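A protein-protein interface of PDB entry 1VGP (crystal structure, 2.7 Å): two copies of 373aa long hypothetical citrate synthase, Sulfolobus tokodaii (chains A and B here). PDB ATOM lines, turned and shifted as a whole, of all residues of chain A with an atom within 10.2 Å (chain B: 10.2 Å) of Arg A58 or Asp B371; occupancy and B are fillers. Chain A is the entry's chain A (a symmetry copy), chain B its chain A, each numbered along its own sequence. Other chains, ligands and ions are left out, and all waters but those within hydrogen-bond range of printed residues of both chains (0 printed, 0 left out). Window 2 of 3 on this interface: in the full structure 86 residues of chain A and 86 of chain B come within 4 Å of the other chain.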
ATOM      1  N   PHE A  40     -24.118   6.590  -2.892  1.00  0.00           N
ATOM      2  CA  PHE A  40     -22.866   7.175  -2.428  1.00  0.00           C
ATOM      3  C   PHE A  40     -22.531   6.880  -0.976  1.00  0.00           C
ATOM      4  O   PHE A  40     -21.389   7.057  -0.549  1.00  0.00           O
ATOM      5  CB  PHE A  40     -22.878   8.689  -2.625  1.00  0.00           C
ATOM      6  CG  PHE A  40     -23.000   9.117  -4.056  1.00  0.00           C
ATOM      7  CD1 PHE A  40     -23.982  10.027  -4.440  1.00  0.00           C
ATOM      8  CD2 PHE A  40     -22.124   8.626  -5.021  1.00  0.00           C
ATOM      9  CE1 PHE A  40     -24.088  10.443  -5.760  1.00  0.00           C
ATOM     10  CE2 PHE A  40     -22.223   9.036  -6.348  1.00  0.00           C
ATOM     11  CZ  PHE A  40     -23.210   9.947  -6.712  1.00  0.00           C
ATOM     12  N   GLU A  45     -22.820   5.254   7.679  1.00  0.00           N
ATOM     13  CA  GLU A  45     -22.939   6.691   7.474  1.00  0.00           C
ATOM     14  C   GLU A  45     -24.393   7.135   7.503  1.00  0.00           C
ATOM     15  O   GLU A  45     -24.721   8.143   8.134  1.00  0.00           O
ATOM     16  CB  GLU A  45     -22.304   7.109   6.150  1.00  0.00           C
ATOM     17  CG  GLU A  45     -22.496   8.580   5.845  1.00  0.00           C
ATOM     18  CD  GLU A  45     -21.699   9.042   4.652  1.00  0.00           C
ATOM     19  OE1 GLU A  45     -22.229   8.941   3.524  1.00  0.00           O
ATOM     20  OE2 GLU A  45     -20.549   9.502   4.838  1.00  0.00           O
ATOM     21  N   TYR A  48     -25.745   7.286  11.066  1.00  0.00           N
ATOM     22  CA  TYR A  48     -25.285   8.494  11.741  1.00  0.00           C
ATOM     23  C   TYR A  48     -26.099   9.706  11.282  1.00  0.00           C
ATOM     24  O   TYR A  48     -26.532  10.523  12.097  1.00  0.00           O
ATOM     25  CB  TYR A  48     -23.797   8.720  11.437  1.00  0.00           C
ATOM     26  CG  TYR A  48     -23.166   9.871  12.193  1.00  0.00           C
ATOM     27  CD1 TYR A  48     -23.461  11.202  11.867  1.00  0.00           C
ATOM     28  CD2 TYR A  48     -22.294   9.631  13.252  1.00  0.00           C
ATOM     29  CE1 TYR A  48     -22.902  12.265  12.585  1.00  0.00           C
ATOM     30  CE2 TYR A  48     -21.731  10.681  13.975  1.00  0.00           C
ATOM     31  CZ  TYR A  48     -22.040  11.997  13.642  1.00  0.00           C
ATOM     32  OH  TYR A  48     -21.518  13.029  14.404  1.00  0.00           O
ATOM     33  N   LYS A  54     -27.088  14.987  10.564  1.00  0.00           N
ATOM     34  CA  LYS A  54     -26.172  15.486   9.544  1.00  0.00           C
ATOM     35  C   LYS A  54     -25.132  14.438   9.165  1.00  0.00           C
ATOM     36  O   LYS A  54     -24.836  13.541   9.955  1.00  0.00           O
ATOM     37  CB  LYS A  54     -25.471  16.762  10.028  1.00  0.00           C
ATOM     38  CG  LYS A  54     -24.787  16.624  11.383  1.00  0.00           C
ATOM     39  CD  LYS A  54     -23.268  16.789  11.281  1.00  0.00           C
ATOM     40  CE  LYS A  54     -22.593  16.555  12.635  1.00  0.00           C
ATOM     41  NZ  LYS A  54     -21.332  17.342  12.790  1.00  0.00           N
ATOM     42  N   LEU A  55     -24.596  14.552   7.950  1.00  0.00           N
ATOM     43  CA  LEU A  55     -23.521  13.677   7.503  1.00  0.00           C
ATOM     44  C   LEU A  55     -22.315  13.914   8.392  1.00  0.00           C
ATOM     45  O   LEU A  55     -21.999  15.060   8.715  1.00  0.00           O
ATOM     46  CB  LEU A  55     -23.159  13.977   6.048  1.00  0.00           C
ATOM     47  CG  LEU A  55     -24.260  13.761   5.004  1.00  0.00           C
ATOM     48  CD1 LEU A  55     -23.874  14.454   3.722  1.00  0.00           C
ATOM     49  CD2 LEU A  55     -24.476  12.268   4.762  1.00  0.00           C
ATOM     50  N   PRO A  56     -21.632  12.834   8.811  1.00  0.00           N
ATOM     51  CA  PRO A  56     -20.472  12.904   9.711  1.00  0.00           C
ATOM     52  C   PRO A  56     -19.213  13.303   8.946  1.00  0.00           C
ATOM     53  O   PRO A  56     -19.063  12.945   7.776  1.00  0.00           O
ATOM     54  CB  PRO A  56     -20.373  11.483  10.243  1.00  0.00           C
ATOM     55  CG  PRO A  56     -20.758  10.673   9.052  1.00  0.00           C
ATOM     56  CD  PRO A  56     -21.904  11.440   8.412  1.00  0.00           C
ATOM     57  N   ASN A  57     -18.305  14.030   9.586  1.00  0.00           N
ATOM     58  CA  ASN A  57     -16.973  14.171   9.014  1.00  0.00           C
ATOM     59  C   ASN A  57     -16.180  12.919   9.350  1.00  0.00           C
ATOM     60  O   ASN A  57     -16.662  12.058  10.081  1.00  0.00           O
ATOM     61  CB  ASN A  57     -16.264  15.414   9.564  1.00  0.00           C
ATOM     62  CG  ASN A  57     -16.090  15.375  11.066  1.00  0.00           C
ATOM     63  OD1 ASN A  57     -15.609  14.390  11.629  1.00  0.00           O
ATOM     64  ND2 ASN A  57     -16.481  16.457  11.728  1.00  0.00           N
ATOM     65  N   ARG A  58     -14.968  12.816   8.818  1.00  0.00           N
ATOM     66  CA  ARG A  58     -14.205  11.577   8.925  1.00  0.00           C
ATOM     67  C   ARG A  58     -13.965  11.139  10.367  1.00  0.00           C
ATOM     68  O   ARG A  58     -13.922   9.941  10.657  1.00  0.00           O
ATOM     69  CB  ARG A  58     -12.871  11.726   8.199  1.00  0.00           C
ATOM     70  CG  ARG A  58     -12.697  10.766   7.032  1.00  0.00           C
ATOM     71  CD  ARG A  58     -12.002  11.457   5.865  1.00  0.00           C
ATOM     72  NE  ARG A  58     -11.780  10.543   4.745  1.00  0.00           N
ATOM     73  CZ  ARG A  58     -11.698  10.929   3.475  1.00  0.00           C
ATOM     74  NH1 ARG A  58     -11.849  12.211   3.157  1.00  0.00           N
ATOM     75  NH2 ARG A  58     -11.466  10.037   2.521  1.00  0.00           N
ATOM     76  N   GLU A  59     -13.805  12.103  11.271  1.00  0.00           N
ATOM     77  CA  GLU A  59     -13.549  11.786  12.672  1.00  0.00           C
ATOM     78  C   GLU A  59     -14.818  11.328  13.376  1.00  0.00           C
ATOM     79  O   GLU A  59     -14.785  10.394  14.181  1.00  0.00           O
ATOM     80  CB  GLU A  59     -12.968  13.001  13.393  1.00  0.00           C
ATOM     81  CG  GLU A  59     -11.843  13.675  12.632  1.00  0.00           C
ATOM     82  CD  GLU A  59     -10.890  14.426  13.539  1.00  0.00           C
ATOM     83  OE1 GLU A  59     -10.007  15.138  13.010  1.00  0.00           O
ATOM     84  OE2 GLU A  59     -11.023  14.305  14.778  1.00  0.00           O
ATOM     85  N   GLU A  60     -15.934  11.986  13.074  1.00  0.00           N
ATOM     86  CA  GLU A  60     -17.206  11.612  13.671  1.00  0.00           C
ATOM     87  C   GLU A  60     -17.619  10.206  13.234  1.00  0.00           C
ATOM     88  O   GLU A  60     -17.946   9.360  14.071  1.00  0.00           O
ATOM     89  CB  GLU A  60     -18.285  12.625  13.302  1.00  0.00           C
ATOM     90  CG  GLU A  60     -18.000  14.021  13.815  1.00  0.00           C
ATOM     91  CD  GLU A  60     -18.976  15.053  13.283  1.00  0.00           C
ATOM     92  OE1 GLU A  60     -19.317  14.991  12.078  1.00  0.00           O
ATOM     93  OE2 GLU A  60     -19.398  15.927  14.071  1.00  0.00           O
ATOM     94  N   LEU A  61     -17.590   9.945  11.932  1.00  0.00           N
ATOM     95  CA  LEU A  61     -17.936   8.620  11.431  1.00  0.00           C
ATOM     96  C   LEU A  61     -16.993   7.549  11.972  1.00  0.00           C
ATOM     97  O   LEU A  61     -17.397   6.410  12.219  1.00  0.00           O
ATOM     98  CB  LEU A  61     -17.896   8.591   9.899  1.00  0.00           C
ATOM     99  CG  LEU A  61     -18.201   7.222   9.273  1.00  0.00           C
ATOM    100  CD1 LEU A  61     -19.639   6.837   9.575  1.00  0.00           C
ATOM    101  CD2 LEU A  61     -17.973   7.269   7.780  1.00  0.00           C
ATOM    102  N   ASN A  62     -15.728   7.915  12.140  1.00  0.00           N
ATOM    103  CA  ASN A  62     -14.726   6.961  12.589  1.00  0.00           C
ATOM    104  C   ASN A  62     -15.046   6.567  14.026  1.00  0.00           C
ATOM    105  O   ASN A  62     -14.952   5.394  14.394  1.00  0.00           O
ATOM    106  CB  ASN A  62     -13.337   7.585  12.508  1.00  0.00           C
ATOM    107  CG  ASN A  62     -12.350   6.699  11.780  1.00  0.00           C
ATOM    108  OD1 ASN A  62     -12.647   6.185  10.696  1.00  0.00           O
ATOM    109  ND2 ASN A  62     -11.169   6.511  12.367  1.00  0.00           N
ATOM    110  N   TRP A  63     -15.432   7.555  14.828  1.00  0.00           N
ATOM    111  CA  TRP A  63     -15.923   7.296  16.163  1.00  0.00           C
ATOM    112  C   TRP A  63     -17.171   6.427  16.107  1.00  0.00           C
ATOM    113  O   TRP A  63     -17.364   5.539  16.937  1.00  0.00           O
ATOM    114  CB  TRP A  63     -16.257   8.609  16.870  1.00  0.00           C
ATOM    115  CG  TRP A  63     -17.036   8.405  18.133  1.00  0.00           C
ATOM    116  CD1 TRP A  63     -16.539   8.061  19.356  1.00  0.00           C
ATOM    117  CD2 TRP A  63     -18.450   8.490  18.289  1.00  0.00           C
ATOM    118  NE1 TRP A  63     -17.554   7.931  20.264  1.00  0.00           N
ATOM    119  CE2 TRP A  63     -18.751   8.195  19.633  1.00  0.00           C
ATOM    120  CE3 TRP A  63     -19.508   8.802  17.422  1.00  0.00           C
ATOM    121  CZ2 TRP A  63     -20.049   8.186  20.139  1.00  0.00           C
ATOM    122  CZ3 TRP A  63     -20.804   8.796  17.918  1.00  0.00           C
ATOM    123  CH2 TRP A  63     -21.063   8.495  19.264  1.00  0.00           C
ATOM    124  N   PHE A  64     -18.021   6.694  15.121  1.00  0.00           N
ATOM    125  CA  PHE A  64     -19.353   6.114  15.098  1.00  0.00           C
ATOM    126  C   PHE A  64     -19.310   4.636  14.758  1.00  0.00           C
ATOM    127  O   PHE A  64     -19.916   3.815  15.440  1.00  0.00           O
ATOM    128  CB  PHE A  64     -20.244   6.841  14.091  1.00  0.00           C
ATOM    129  CG  PHE A  64     -21.626   6.271  14.002  1.00  0.00           C
ATOM    130  CD1 PHE A  64     -22.549   6.494  15.014  1.00  0.00           C
ATOM    131  CD2 PHE A  64     -21.997   5.477  12.920  1.00  0.00           C
ATOM    132  CE1 PHE A  64     -23.822   5.935  14.956  1.00  0.00           C
ATOM    133  CE2 PHE A  64     -23.270   4.911  12.853  1.00  0.00           C
ATOM    134  CZ  PHE A  64     -24.183   5.141  13.873  1.00  0.00           C
ATOM    135  N   GLN A  65     -18.593   4.288  13.699  1.00  0.00           N
ATOM    136  CA  GLN A  65     -18.477   2.886  13.333  1.00  0.00           C
ATOM    137  C   GLN A  65     -17.514   2.159  14.252  1.00  0.00           C
ATOM    138  O   GLN A  65     -17.381   0.946  14.178  1.00  0.00           O
ATOM    139  CB  GLN A  65     -18.035   2.739  11.876  1.00  0.00           C
ATOM    140  CG  GLN A  65     -16.818   3.541  11.491  1.00  0.00           C
ATOM    141  CD  GLN A  65     -16.737   3.787   9.995  1.00  0.00           C
ATOM    142  OE1 GLN A  65     -15.662   4.043   9.458  1.00  0.00           O
ATOM    143  NE2 GLN A  65     -17.878   3.712   9.315  1.00  0.00           N
ATOM    144  N   GLU A  66     -16.842   2.894  15.124  1.00  0.00           N
ATOM    145  CA  GLU A  66     -16.024   2.260  16.148  1.00  0.00           C
ATOM    146  C   GLU A  66     -16.942   1.674  17.221  1.00  0.00           C
ATOM    147  O   GLU A  66     -16.797   0.518  17.608  1.00  0.00           O
ATOM    148  CB  GLU A  66     -15.071   3.300  16.751  1.00  0.00           C
ATOM    149  CG  GLU A  66     -14.706   3.089  18.217  1.00  0.00           C
ATOM    150  CD  GLU A  66     -13.291   3.554  18.549  1.00  0.00           C
ATOM    151  OE1 GLU A  66     -12.846   4.578  17.966  1.00  0.00           O
ATOM    152  OE2 GLU A  66     -12.630   2.900  19.386  1.00  0.00           O
ATOM    153  N   TYR B 367     -25.681  15.912  -1.668  1.00  0.00           N
ATOM    154  CA  TYR B 367     -24.836  14.980  -0.924  1.00  0.00           C
ATOM    155  C   TYR B 367     -23.393  15.404  -1.035  1.00  0.00           C
ATOM    156  O   TYR B 367     -22.804  15.326  -2.112  1.00  0.00           O
ATOM    157  CB  TYR B 367     -24.956  13.554  -1.471  1.00  0.00           C
ATOM    158  CG  TYR B 367     -23.995  12.577  -0.806  1.00  0.00           C
ATOM    159  CD1 TYR B 367     -24.326  11.956   0.403  1.00  0.00           C
ATOM    160  CD2 TYR B 367     -22.743  12.303  -1.361  1.00  0.00           C
ATOM    161  CE1 TYR B 367     -23.443  11.096   1.040  1.00  0.00           C
ATOM    162  CE2 TYR B 367     -21.848  11.435  -0.723  1.00  0.00           C
ATOM    163  CZ  TYR B 367     -22.209  10.841   0.479  1.00  0.00           C
ATOM    164  OH  TYR B 367     -21.332  10.011   1.132  1.00  0.00           O
ATOM    165  N   ILE B 368     -22.810  15.843   0.068  1.00  0.00           N
ATOM    166  CA  ILE B 368     -21.446  16.327   0.012  1.00  0.00           C
ATOM    167  C   ILE B 368     -20.481  15.225   0.422  1.00  0.00           C
ATOM    168  O   ILE B 368     -20.697  14.534   1.417  1.00  0.00           O
ATOM    169  CB  ILE B 368     -21.259  17.578   0.912  1.00  0.00           C
ATOM    170  CG1 ILE B 368     -19.789  17.724   1.293  1.00  0.00           C
ATOM    171  CG2 ILE B 368     -22.150  17.486   2.145  1.00  0.00           C
ATOM    172  CD1 ILE B 368     -19.522  18.856   2.275  1.00  0.00           C
ATOM    173  N   PRO B 369     -19.410  15.030  -0.368  1.00  0.00           N
ATOM    174  CA  PRO B 369     -18.376  14.020  -0.106  1.00  0.00           C
ATOM    175  C   PRO B 369     -17.685  14.259   1.222  1.00  0.00           C
ATOM    176  O   PRO B 369     -17.552  15.399   1.670  1.00  0.00           O
ATOM    177  CB  PRO B 369     -17.410  14.186  -1.277  1.00  0.00           C
ATOM    178  CG  PRO B 369     -18.240  14.772  -2.354  1.00  0.00           C
ATOM    179  CD  PRO B 369     -19.149  15.730  -1.637  1.00  0.00           C
ATOM    180  N   ILE B 370     -17.234  13.180   1.845  1.00  0.00           N
ATOM    181  CA  ILE B 370     -16.828  13.252   3.232  1.00  0.00           C
ATOM    182  C   ILE B 370     -15.589  14.132   3.445  1.00  0.00           C
ATOM    183  O   ILE B 370     -15.515  14.839   4.444  1.00  0.00           O
ATOM    184  CB  ILE B 370     -16.605  11.839   3.800  1.00  0.00           C
ATOM    185  CG1 ILE B 370     -16.468  11.896   5.323  1.00  0.00           C
ATOM    186  CG2 ILE B 370     -15.407  11.204   3.152  1.00  0.00           C
ATOM    187  CD1 ILE B 370     -16.798  10.585   5.999  1.00  0.00           C
ATOM    188  N   ASP B 371     -14.633  14.138   2.514  1.00  0.00           N
ATOM    189  CA  ASP B 371     -13.522  15.066   2.689  1.00  0.00           C
ATOM    190  C   ASP B 371     -13.960  16.536   2.607  1.00  0.00           C
ATOM    191  O   ASP B 371     -13.439  17.370   3.346  1.00  0.00           O
ATOM    192  CB  ASP B 371     -12.349  14.790   1.726  1.00  0.00           C
ATOM    193  CG  ASP B 371     -12.785  14.414   0.316  1.00  0.00           C
ATOM    194  OD1 ASP B 371     -12.336  15.109  -0.638  1.00  0.00           O
ATOM    195  OD2 ASP B 371     -13.551  13.440   0.149  1.00  0.00           O
ATOM    196  N   SER B 372     -14.935  16.857   1.759  1.00  0.00           N
ATOM    197  CA  SER B 372     -15.425  18.233   1.674  1.00  0.00           C
ATOM    198  C   SER B 372     -16.246  18.677   2.885  1.00  0.00           C
ATOM    199  O   SER B 372     -16.738  19.806   2.925  1.00  0.00           O
ATOM    200  CB  SER B 372     -16.272  18.422   0.414  1.00  0.00           C
ATOM    201  OG  SER B 372     -15.538  18.066  -0.741  1.00  0.00           O
ATOM    202  N   ARG B 373     -16.391  17.793   3.868  1.00  0.00           N
ATOM    203  CA  ARG B 373     -17.262  18.056   5.014  1.00  0.00           C
ATOM    204  C   ARG B 373     -16.513  18.733   6.161  1.00  0.00           C
ATOM    205  O   ARG B 373     -17.108  19.624   6.809  1.00  0.00           O
ATOM    206  CB  ARG B 373     -17.889  16.748   5.513  1.00  0.00           C
ATOM    207  CG  ARG B 373     -18.977  16.202   4.605  1.00  0.00           C
ATOM    208  CD  ARG B 373     -19.505  14.873   5.104  1.00  0.00           C
ATOM    209  NE  ARG B 373     -20.030  14.062   4.012  1.00  0.00           N
ATOM    210  CZ  ARG B 373     -20.249  12.751   4.092  1.00  0.00           C
ATOM    211  NH1 ARG B 373     -20.617  12.071   3.013  1.00  0.00           N
ATOM    212  NH2 ARG B 373     -20.100  12.117   5.250  1.00  0.00           N
ATOM    213  OXT ARG B 373     -15.341  18.359   6.402  1.00  0.00           O
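OE1 of Glu A45 lies within hydrogen-bond range of OH of Tyr B367, 2.8 Å away.
OH of Tyr B367 sits at hydrogen-bond distance from O of Phe A40 (3.4 Å).
OE2 of Glu A45 lies within salt-bridge range of NH2 of Arg B373, at 2.7 Å.
The guanidinium group (NH2) of Arg B373 sits at hydrogen-bond distance from the backbone carbonyl oxygen (O) of Pro A56.
The side-chain carboxylate of Asp B371 is in salt-bridge range of the guanidinium group of Arg A58, at 3.7 Å.
NH1 of Arg B373 is in hydrogen-bond range of OH of Tyr B367 (2.9 Å).
The backbone carbonyl oxygen (O) of Ile B368 sits at hydrogen-bond distance from the guanidinium group (NE) of Arg B373 (2.7 Å).
Ile B368 touches Leu A55 (CG2 to CD1, 3.8 Å).
Arg B373 touches Leu A55 (NH2 to CB, 3.7 Å).
Ile B370 touches Pro A56 (CG1 to O, 3.7 Å).
Arg A58 touches Ile B370 (NH1 to CG2, 3.7 Å).
CD2 of Leu A61 touches CD1 of Ile B370 (3.9 Å).
Arg A58 touches two residues of chain B.
Of chain A, only Arg A58 (3.0 Å) comes within 4 Å of Asp B371.
No residue of chain B comes within 4 Å of Asn A57.
Ile B370 touches three residues of chain A.
No residue of chain A comes within 4 Å of Ser B372.
Of the printed residues of chain B, Leu A61 touches Ile B370.
Printed residues of chain B within 4 Å of Leu A55: Ile B368 and Arg B373.
Of the printed residues of chain B, Glu A45 touches Tyr B367 (2.8 Å) and Arg B373 (2.7 Å).
Printed residues of chain A within 4 Å of Ile B368: Leu A55 (3.8 Å).
Glu A66 touches none of the printed residues of chain B.
The nearest residue of chain A that does not touch Asp B371 is Asn A57 (6.9 Å).
Hydrophobic or aromatic side chains of chain A that line the printed part of chain B: Phe A40, Leu A55, Pro A56 and Leu A61.
Among the printed residues, 10 pairs touch across the chains.
No position is printed for both chains.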
